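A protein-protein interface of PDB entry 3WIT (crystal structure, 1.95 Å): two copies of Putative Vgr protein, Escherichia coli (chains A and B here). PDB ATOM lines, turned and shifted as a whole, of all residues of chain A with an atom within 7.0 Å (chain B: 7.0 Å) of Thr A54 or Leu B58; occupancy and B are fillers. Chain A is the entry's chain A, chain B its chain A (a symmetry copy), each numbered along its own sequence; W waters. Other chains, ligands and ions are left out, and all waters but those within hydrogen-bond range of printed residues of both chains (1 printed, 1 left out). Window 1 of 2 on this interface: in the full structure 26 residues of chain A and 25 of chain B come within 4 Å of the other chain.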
ATOM      1  N   GLU A  36      -1.283  22.227  -5.950  1.00  0.00           N
ATOM      2  CA  GLU A  36      -0.926  21.997  -7.356  1.00  0.00           C
ATOM      3  C   GLU A  36      -1.479  20.715  -7.979  1.00  0.00           C
ATOM      4  O   GLU A  36      -1.182  20.391  -9.143  1.00  0.00           O
ATOM      5  CB  GLU A  36       0.601  22.073  -7.536  1.00  0.00           C
ATOM      6  CG  GLU A  36       1.129  23.458  -7.313  1.00  0.00           C
ATOM      7  CD  GLU A  36       0.237  24.485  -7.986  1.00  0.00           C
ATOM      8  OE1 GLU A  36       0.070  24.396  -9.228  1.00  0.00           O
ATOM      9  OE2 GLU A  36      -0.324  25.357  -7.279  1.00  0.00           O
ATOM     10  N   SER A  37      -2.291  19.983  -7.215  1.00  0.00           N
ATOM     11  CA  SER A  37      -2.925  18.776  -7.729  1.00  0.00           C
ATOM     12  C   SER A  37      -4.359  19.101  -8.125  1.00  0.00           C
ATOM     13  O   SER A  37      -5.133  19.606  -7.301  1.00  0.00           O
ATOM     14  CB  SER A  37      -2.911  17.681  -6.663  1.00  0.00           C
ATOM     15  OG  SER A  37      -1.682  17.696  -5.939  1.00  0.00           O
ATOM     16  N   LYS A  38      -4.715  18.822  -9.376  1.00  0.00           N
ATOM     17  CA  LYS A  38      -6.019  19.239  -9.905  1.00  0.00           C
ATOM     18  C   LYS A  38      -6.601  18.193 -10.808  1.00  0.00           C
ATOM     19  O   LYS A  38      -5.871  17.541 -11.561  1.00  0.00           O
ATOM     20  CB  LYS A  38      -5.877  20.524 -10.728  1.00  0.00           C
ATOM     21  CG  LYS A  38      -5.333  21.710  -9.997  1.00  0.00           C
ATOM     22  CD  LYS A  38      -5.431  22.938 -10.904  1.00  0.00           C
ATOM     23  CE  LYS A  38      -5.134  24.220 -10.153  1.00  0.00           C
ATOM     24  NZ  LYS A  38      -3.756  24.242  -9.588  1.00  0.00           N
ATOM     25  N   GLN A  47      -8.733  16.758 -17.418  1.00  0.00           N
ATOM     26  CA  GLN A  47      -7.288  16.868 -17.168  1.00  0.00           C
ATOM     27  C   GLN A  47      -6.983  16.590 -15.704  1.00  0.00           C
ATOM     28  O   GLN A  47      -7.646  17.127 -14.820  1.00  0.00           O
ATOM     29  CB  GLN A  47      -6.794  18.251 -17.556  1.00  0.00           C
ATOM     30  CG  GLN A  47      -5.296  18.417 -17.388  1.00  0.00           C
ATOM     31  CD  GLN A  47      -4.763  19.471 -18.298  1.00  0.00           C
ATOM     32  OE1 GLN A  47      -5.028  19.459 -19.494  1.00  0.00           O
ATOM     33  NE2 GLN A  47      -4.034  20.417 -17.737  1.00  0.00           N
ATOM     34  N   LEU A  48      -5.985  15.738 -15.464  1.00  0.00           N
ATOM     35  CA  LEU A  48      -5.471  15.470 -14.141  1.00  0.00           C
ATOM     36  C   LEU A  48      -4.025  15.914 -14.154  1.00  0.00           C
ATOM     37  O   LEU A  48      -3.275  15.549 -15.068  1.00  0.00           O
ATOM     38  CB  LEU A  48      -5.563  13.971 -13.832  1.00  0.00           C
ATOM     39  CG  LEU A  48      -6.919  13.253 -13.995  1.00  0.00           C
ATOM     40  CD1 LEU A  48      -7.106  12.632 -15.375  1.00  0.00           C
ATOM     41  CD2 LEU A  48      -7.069  12.148 -12.941  1.00  0.00           C
ATOM     42  N   GLN A  49      -3.618  16.706 -13.162  1.00  0.00           N
ATOM     43  CA  GLN A  49      -2.242  17.181 -13.140  1.00  0.00           C
ATOM     44  C   GLN A  49      -1.752  17.441 -11.757  1.00  0.00           C
ATOM     45  O   GLN A  49      -2.531  17.723 -10.834  1.00  0.00           O
ATOM     46  CB  GLN A  49      -2.080  18.465 -13.941  1.00  0.00           C
ATOM     47  CG  GLN A  49      -2.952  19.574 -13.471  1.00  0.00           C
ATOM     48  CD  GLN A  49      -2.901  20.745 -14.426  1.00  0.00           C
ATOM     49  OE1 GLN A  49      -3.932  21.189 -14.934  1.00  0.00           O
ATOM     50  NE2 GLN A  49      -1.691  21.234 -14.701  1.00  0.00           N
ATOM     51  N   VAL A  50      -0.436  17.371 -11.624  1.00  0.00           N
ATOM     52  CA  VAL A  50       0.229  17.655 -10.368  1.00  0.00           C
ATOM     53  C   VAL A  50       1.458  18.460 -10.716  1.00  0.00           C
ATOM     54  O   VAL A  50       2.356  17.986 -11.432  1.00  0.00           O
ATOM     55  CB  VAL A  50       0.651  16.392  -9.628  1.00  0.00           C
ATOM     56  CG1 VAL A  50       1.348  16.770  -8.344  1.00  0.00           C
ATOM     57  CG2 VAL A  50      -0.588  15.497  -9.339  1.00  0.00           C
ATOM     58  N   GLY A  51       1.505  19.683 -10.216  1.00  0.00           N
ATOM     59  CA  GLY A  51       2.617  20.582 -10.531  1.00  0.00           C
ATOM     60  C   GLY A  51       2.558  20.909 -12.011  1.00  0.00           C
ATOM     61  O   GLY A  51       1.512  20.752 -12.653  1.00  0.00           O
ATOM     62  N   GLU A  52       3.678  21.294 -12.603  1.00  0.00           N
ATOM     63  CA  GLU A  52       3.552  21.793 -13.967  1.00  0.00           C
ATOM     64  C   GLU A  52       3.841  20.774 -15.056  1.00  0.00           C
ATOM     65  O   GLU A  52       3.549  21.013 -16.220  1.00  0.00           O
ATOM     66  CB  GLU A  52       4.358  23.081 -14.183  1.00  0.00           C
ATOM     67  CG  GLU A  52       3.749  24.003 -15.268  1.00  0.00           C
ATOM     68  CD  GLU A  52       2.308  24.443 -14.962  1.00  0.00           C
ATOM     69  OE1 GLU A  52       1.419  24.256 -15.827  1.00  0.00           O
ATOM     70  OE2 GLU A  52       2.065  24.990 -13.862  1.00  0.00           O
ATOM     71  N   SER A  53       4.384  19.623 -14.697  1.00  0.00           N
ATOM     72  CA  SER A  53       4.806  18.723 -15.748  1.00  0.00           C
ATOM     73  C   SER A  53       4.288  17.306 -15.644  1.00  0.00           C
ATOM     74  O   SER A  53       4.622  16.473 -16.465  1.00  0.00           O
ATOM     75  CB  SER A  53       6.331  18.741 -15.893  1.00  0.00           C
ATOM     76  OG  SER A  53       6.950  18.244 -14.728  1.00  0.00           O
ATOM     77  N   THR A  54       3.476  17.008 -14.648  1.00  0.00           N
ATOM     78  CA  THR A  54       2.839  15.693 -14.627  1.00  0.00           C
ATOM     79  C   THR A  54       1.405  15.898 -15.062  1.00  0.00           C
ATOM     80  O   THR A  54       0.644  16.601 -14.368  1.00  0.00           O
ATOM     81  CB  THR A  54       2.845  15.129 -13.208  1.00  0.00           C
ATOM     82  OG1 THR A  54       4.205  14.969 -12.763  1.00  0.00           O
ATOM     83  CG2 THR A  54       2.085  13.788 -13.145  1.00  0.00           C
ATOM     84  N   VAL A  55       1.015  15.325 -16.202  1.00  0.00           N
ATOM     85  CA  VAL A  55      -0.346  15.564 -16.725  1.00  0.00           C
ATOM     86  C   VAL A  55      -0.932  14.373 -17.454  1.00  0.00           C
ATOM     87  O   VAL A  55      -0.264  13.775 -18.295  1.00  0.00           O
ATOM     88  CB  VAL A  55      -0.372  16.703 -17.776  1.00  0.00           C
ATOM     89  CG1 VAL A  55      -1.804  16.956 -18.225  1.00  0.00           C
ATOM     90  CG2 VAL A  55       0.249  17.986 -17.264  1.00  0.00           C
ATOM     91  N   ILE A  56      -2.171  14.017 -17.140  1.00  0.00           N
ATOM     92  CA  ILE A  56      -2.940  13.126 -17.998  1.00  0.00           C
ATOM     93  C   ILE A  56      -4.109  13.922 -18.551  1.00  0.00           C
ATOM     94  O   ILE A  56      -4.906  14.475 -17.790  1.00  0.00           O
ATOM     95  CB  ILE A  56      -3.462  11.913 -17.237  1.00  0.00           C
ATOM     96  CG1 ILE A  56      -2.282  11.090 -16.728  1.00  0.00           C
ATOM     97  CG2 ILE A  56      -4.388  11.061 -18.138  1.00  0.00           C
ATOM     98  CD1 ILE A  56      -2.672   9.961 -15.824  1.00  0.00           C
ATOM     99  N   ILE A  65      -0.325  11.312 -21.789  1.00  0.00           N
ATOM    100  CA  ILE A  65       0.178  11.041 -20.438  1.00  0.00           C
ATOM    101  C   ILE A  65       1.622  11.523 -20.468  1.00  0.00           C
ATOM    102  O   ILE A  65       2.362  11.103 -21.348  1.00  0.00           O
ATOM    103  CB  ILE A  65       0.170   9.526 -20.130  1.00  0.00           C
ATOM    104  CG1 ILE A  65      -1.262   8.995 -20.156  1.00  0.00           C
ATOM    105  CG2 ILE A  65       0.841   9.220 -18.763  1.00  0.00           C
ATOM    106  CD1 ILE A  65      -1.383   7.497 -20.074  1.00  0.00           C
ATOM    107  N   VAL A  66       2.009  12.439 -19.567  1.00  0.00           N
ATOM    108  CA  VAL A  66       3.411  12.913 -19.468  1.00  0.00           C
ATOM    109  C   VAL A  66       3.801  12.995 -17.973  1.00  0.00           C
ATOM    110  O   VAL A  66       2.980  13.363 -17.120  1.00  0.00           O
ATOM    111  CB  VAL A  66       3.660  14.286 -20.120  1.00  0.00           C
ATOM    112  CG1 VAL A  66       3.398  14.249 -21.609  1.00  0.00           C
ATOM    113  CG2 VAL A  66       2.782  15.336 -19.500  1.00  0.00           C
ATOM    114  N   GLY A  67       5.043  12.633 -17.670  1.00  0.00           N
ATOM    115  CA  GLY A  67       5.573  12.701 -16.318  1.00  0.00           C
ATOM    116  C   GLY A  67       7.083  12.629 -16.362  1.00  0.00           C
ATOM    117  O   GLY A  67       7.643  12.000 -17.268  1.00  0.00           O
ATOM    118  N   GLY A  68       7.766  13.254 -15.404  1.00  0.00           N
ATOM    119  CA  GLY A  68       9.225  13.233 -15.424  1.00  0.00           C
ATOM    120  C   GLY A  68       9.702  11.786 -15.505  1.00  0.00           C
ATOM    121  O   GLY A  68      10.596  11.436 -16.279  1.00  0.00           O
ATOM    122  N   SER A  69       9.096  10.933 -14.696  1.00  0.00           N
ATOM    123  CA  SER A  69       9.312   9.500 -14.821  1.00  0.00           C
ATOM    124  C   SER A  69       7.960   8.883 -14.945  1.00  0.00           C
ATOM    125  O   SER A  69       7.072   9.190 -14.149  1.00  0.00           O
ATOM    126  CB  SER A  69       9.994   8.965 -13.567  1.00  0.00           C
ATOM    127  OG  SER A  69      11.276   9.529 -13.470  1.00  0.00           O
ATOM    128  N   ASP B  44       0.558  16.341  -2.218  1.00  0.00           N
ATOM    129  CA  ASP B  44       1.588  15.464  -2.777  1.00  0.00           C
ATOM    130  C   ASP B  44       1.221  14.909  -4.130  1.00  0.00           C
ATOM    131  O   ASP B  44       2.098  14.434  -4.871  1.00  0.00           O
ATOM    132  CB  ASP B  44       1.820  14.285  -1.866  1.00  0.00           C
ATOM    133  CG  ASP B  44       2.743  14.612  -0.726  1.00  0.00           C
ATOM    134  OD1 ASP B  44       3.341  15.719  -0.706  1.00  0.00           O
ATOM    135  OD2 ASP B  44       2.886  13.735   0.147  1.00  0.00           O
ATOM    136  N   GLY B  45      -0.068  14.921  -4.451  1.00  0.00           N
ATOM    137  CA  GLY B  45      -0.488  14.484  -5.779  1.00  0.00           C
ATOM    138  C   GLY B  45      -1.869  13.864  -5.817  1.00  0.00           C
ATOM    139  O   GLY B  45      -2.748  14.187  -5.002  1.00  0.00           O
ATOM    140  N   ILE B  46      -2.060  12.935  -6.744  1.00  0.00           N
ATOM    141  CA  ILE B  46      -3.370  12.349  -6.971  1.00  0.00           C
ATOM    142  C   ILE B  46      -3.206  10.844  -7.007  1.00  0.00           C
ATOM    143  O   ILE B  46      -2.260  10.324  -7.607  1.00  0.00           O
ATOM    144  CB  ILE B  46      -3.960  12.829  -8.313  1.00  0.00           C
ATOM    145  CG1 ILE B  46      -4.071  14.359  -8.316  1.00  0.00           C
ATOM    146  CG2 ILE B  46      -5.299  12.110  -8.603  1.00  0.00           C
ATOM    147  CD1 ILE B  46      -4.600  14.985  -9.662  1.00  0.00           C
ATOM    148  N   GLN B  47      -4.088  10.134  -6.322  1.00  0.00           N
ATOM    149  CA  GLN B  47      -4.078   8.669  -6.444  1.00  0.00           C
ATOM    150  C   GLN B  47      -5.468   8.159  -6.794  1.00  0.00           C
ATOM    151  O   GLN B  47      -6.450   8.564  -6.177  1.00  0.00           O
ATOM    152  CB  GLN B  47      -3.596   8.039  -5.148  1.00  0.00           C
ATOM    153  CG  GLN B  47      -3.495   6.529  -5.222  1.00  0.00           C
ATOM    154  CD  GLN B  47      -2.497   6.004  -4.248  1.00  0.00           C
ATOM    155  OE1 GLN B  47      -1.366   6.473  -4.195  1.00  0.00           O
ATOM    156  NE2 GLN B  47      -2.911   5.047  -3.438  1.00  0.00           N
ATOM    157  N   LEU B  48      -5.536   7.281  -7.796  1.00  0.00           N
ATOM    158  CA  LEU B  48      -6.749   6.592  -8.166  1.00  0.00           C
ATOM    159  C   LEU B  48      -6.478   5.119  -7.955  1.00  0.00           C
ATOM    160  O   LEU B  48      -5.449   4.608  -8.415  1.00  0.00           O
ATOM    161  CB  LEU B  48      -7.083   6.864  -9.638  1.00  0.00           C
ATOM    162  CG  LEU B  48      -7.169   8.323 -10.131  1.00  0.00           C
ATOM    163  CD1 LEU B  48      -5.849   8.845 -10.689  1.00  0.00           C
ATOM    164  CD2 LEU B  48      -8.242   8.457 -11.219  1.00  0.00           C
ATOM    165  N   ILE B  56      -3.228   4.141 -10.062  1.00  0.00           N
ATOM    166  CA  ILE B  56      -2.528   5.180 -10.805  1.00  0.00           C
ATOM    167  C   ILE B  56      -2.183   6.287  -9.826  1.00  0.00           C
ATOM    168  O   ILE B  56      -3.068   6.841  -9.169  1.00  0.00           O
ATOM    169  CB  ILE B  56      -3.380   5.744 -11.935  1.00  0.00           C
ATOM    170  CG1 ILE B  56      -3.680   4.638 -12.942  1.00  0.00           C
ATOM    171  CG2 ILE B  56      -2.664   6.936 -12.614  1.00  0.00           C
ATOM    172  CD1 ILE B  56      -4.649   5.036 -14.013  1.00  0.00           C
ATOM    173  N   ARG B  57      -0.897   6.582  -9.698  1.00  0.00           N
ATOM    174  CA  ARG B  57      -0.458   7.662  -8.834  1.00  0.00           C
ATOM    175  C   ARG B  57       0.252   8.743  -9.651  1.00  0.00           C
ATOM    176  O   ARG B  57       1.130   8.450 -10.472  1.00  0.00           O
ATOM    177  CB  ARG B  57       0.488   7.117  -7.772  1.00  0.00           C
ATOM    178  CG  ARG B  57       1.214   8.229  -7.067  1.00  0.00           C
ATOM    179  CD  ARG B  57       0.600   8.545  -5.726  1.00  0.00           C
ATOM    180  NE  ARG B  57       1.580   8.316  -4.667  1.00  0.00           N
ATOM    181  CZ  ARG B  57       2.066   7.119  -4.344  1.00  0.00           C
ATOM    182  NH1 ARG B  57       1.656   6.029  -4.996  1.00  0.00           N
ATOM    183  NH2 ARG B  57       2.967   7.009  -3.366  1.00  0.00           N
ATOM    184  N   LEU B  58      -0.126   9.989  -9.415  1.00  0.00           N
ATOM    185  CA  LEU B  58       0.521  11.133 -10.036  1.00  0.00           C
ATOM    186  C   LEU B  58       1.172  11.968  -8.949  1.00  0.00           C
ATOM    187  O   LEU B  58       0.525  12.283  -7.928  1.00  0.00           O
ATOM    188  CB  LEU B  58      -0.539  11.986 -10.751  1.00  0.00           C
ATOM    189  CG  LEU B  58      -1.235  11.446 -12.008  1.00  0.00           C
ATOM    190  CD1 LEU B  58      -2.348  10.480 -11.683  1.00  0.00           C
ATOM    191  CD2 LEU B  58      -1.794  12.644 -12.792  1.00  0.00           C
ATOM    192  N   SER B  59       2.427  12.349  -9.160  1.00  0.00           N
ATOM    193  CA  SER B  59       3.143  13.182  -8.198  1.00  0.00           C
ATOM    194  C   SER B  59       3.857  14.230  -9.009  1.00  0.00           C
ATOM    195  O   SER B  59       3.825  14.181 -10.232  1.00  0.00           O
ATOM    196  CB  SER B  59       4.171  12.355  -7.466  1.00  0.00           C
ATOM    197  OG  SER B  59       5.339  12.212  -8.263  1.00  0.00           O
ATOM    198  N   LYS B  60       4.539  15.149  -8.338  1.00  0.00           N
ATOM    199  CA  LYS B  60       5.289  16.205  -9.020  1.00  0.00           C
ATOM    200  C   LYS B  60       6.339  15.637  -9.976  1.00  0.00           C
ATOM    201  O   LYS B  60       6.697  16.274 -10.970  1.00  0.00           O
ATOM    202  CB  LYS B  60       5.978  17.108  -7.994  1.00  0.00           C
ATOM    203  CG  LYS B  60       5.366  18.502  -7.884  1.00  0.00           C
ATOM    204  CD  LYS B  60       5.223  18.972  -6.421  1.00  0.00           C
ATOM    205  CE  LYS B  60       3.746  19.123  -6.001  1.00  0.00           C
ATOM    206  NZ  LYS B  60       3.456  18.562  -4.638  1.00  0.00           N
ATOM    207  N   ASP B  61       6.843  14.450  -9.651  1.00  0.00           N
ATOM    208  CA  ASP B  61       7.968  13.860 -10.363  1.00  0.00           C
ATOM    209  C   ASP B  61       7.576  12.835 -11.438  1.00  0.00           C
ATOM    210  O   ASP B  61       8.411  12.442 -12.266  1.00  0.00           O
ATOM    211  CB  ASP B  61       8.911  13.200  -9.375  1.00  0.00           C
ATOM    212  CG  ASP B  61       9.518  14.194  -8.405  1.00  0.00           C
ATOM    213  OD1 ASP B  61       9.843  15.333  -8.825  1.00  0.00           O
ATOM    214  OD2 ASP B  61       9.666  13.832  -7.220  1.00  0.00           O
ATOM    215  N   GLY B  62       6.341  12.396 -11.442  1.00  0.00           N
ATOM    216  CA  GLY B  62       5.937  11.473 -12.498  1.00  0.00           C
ATOM    217  C   GLY B  62       4.683  10.697 -12.199  1.00  0.00           C
ATOM    218  O   GLY B  62       3.841  11.122 -11.413  1.00  0.00           O
ATOM    219  N   ILE B  63       4.542   9.550 -12.850  1.00  0.00           N
ATOM    220  CA  ILE B  63       3.287   8.819 -12.811  1.00  0.00           C
ATOM    221  C   ILE B  63       3.647   7.357 -12.681  1.00  0.00           C
ATOM    222  O   ILE B  63       4.579   6.877 -13.357  1.00  0.00           O
ATOM    223  CB  ILE B  63       2.493   9.017 -14.144  1.00  0.00           C
ATOM    224  CG1 ILE B  63       2.101  10.477 -14.323  1.00  0.00           C
ATOM    225  CG2 ILE B  63       1.243   8.145 -14.189  1.00  0.00           C
ATOM    226  CD1 ILE B  63       1.387  10.792 -15.649  1.00  0.00           C
ATOM    227  N   THR B  64       2.935   6.643 -11.814  1.00  0.00           N
ATOM    228  CA  THR B  64       3.059   5.184 -11.791  1.00  0.00           C
ATOM    229  C   THR B  64       1.686   4.607 -12.077  1.00  0.00           C
ATOM    230  O   THR B  64       0.666   5.131 -11.608  1.00  0.00           O
ATOM    231  CB  THR B  64       3.700   4.618 -10.458  1.00  0.00           C
ATOM    232  OG1 THR B  64       2.842   4.879  -9.352  1.00  0.00           O
ATOM    233  CG2 THR B  64       5.052   5.240 -10.170  1.00  0.00           C
HETATM  234  O   HOH W   1       6.582  15.340 -13.830  1.00  0.00           O
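The backbone carbonyl oxygen of Ser B59 lies within hydrogen-bond range of the side-chain hydroxyl of Thr A54.
OG1 of Thr A54 sits at hydrogen-bond distance from O of Lys B60, 3.3 Å away.
O of Asp B61 lies within hydrogen-bond range of N of Gly A68 (3.3 Å).
The backbone NH of Ser A69 is in hydrogen-bond range of the backbone carbonyl oxygen of Asp B61 (2.9 Å).
The backbone NH of Ile B63 is in hydrogen-bond range of the backbone carbonyl oxygen of Ser A69 (2.9 Å).
Of the 14 printed residues of chain B, 8 touch a printed residue of chain A.
Hydrophobic or aromatic side chains of chain B that line the printed part of chain A: Ile B46, Leu B58 and Ile B63.
Among the printed residues, 23 pairs touch across the chains.
Among the printed residues, no Asp or Glu carboxylate lies within 4 Å of a Lys or Arg side-chain nitrogen of the other chain.
The side-chain amide nitrogen of Gln A47 is in hydrogen-bond range of the side-chain amide oxygen of Gln A49, at 2.9 Å.
The backbone carbonyl oxygen of Leu A48 sits at hydrogen-bond distance from the backbone NH of Ile A56, at 2.8 Å.
The backbone carbonyl oxygen of Val A66 lies within hydrogen-bond range of the backbone NH of Val A55 (2.9 Å).
O of Ile B46 is in hydrogen-bond range of N of Leu B58.
The side-chain hydroxyl (OG) of Ser B59 sits at hydrogen-bond distance from the backbone NH (N) of Asp B61 (3.0 Å).
The side-chain hydroxyl (OG) of Ser B59 sits at hydrogen-bond distance from the backbone NH (N) of Gly B62 (3.3 Å).
Among the printed residues, merely in contact across the chains: Ser A69 with Gly B62 (3.0 Å), Val A66 with Ile B63 (3.4 Å), Lys A38 with Ile B46 (3.4 Å), Ser A37 with Gly B45 (3.4 Å), Thr A54 with Ile B63 (3.5 Å), Ile A65 with Ile B63 (3.5 Å), Val A50 with Lys B60 (3.6 Å), Thr A54 with Gly B62 (3.6 Å), Gln A49 with Ile B46 (3.6 Å), Val A50 with Ser B59 (3.6 Å), Val A50 with Leu B58 (3.7 Å), Val A50 with Gly B45 (3.7 Å), Val A50 with Ile B46 (3.8 Å), Ile A56 with Ile B63 (3.8 Å), Gly A68 with Gly B62 (3.9 Å), Ser A37 with Ile B46 (3.9 Å), Leu A48 with Leu B58 (3.98 Å) and Thr A54 with Leu B58 (3.98 Å).
Water W1 lies within hydrogen-bond range of OG1 of Thr A54, N of Gly A68, O of Lys B60 and OG of Ser A53.
3 positions are printed for both chains.
Glu A36 touches none of the printed residues of chain B.
Of the printed residues of chain B, Thr A54 touches Leu B58 (3.98 Å), Ser B59 (2.7 Å), Lys B60 (3.3 Å), Gly B62 (3.6 Å) and Ile B63 (3.5 Å).
Val A55 touches none of the printed residues of chain B.
Of the printed residues of chain A, Gly B45 touches Ser A37 (3.4 Å) and Val A50 (3.7 Å).
Printed residues of chain A within 4 Å of Lys B60: Val A50 and Thr A54.
The nearest printed residue of chain A that does not touch Leu B58 is Ile A56 (4.1 Å).
The nearest printed residue of chain B that does not touch Ser A69 is Thr B64 (5.4 Å).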
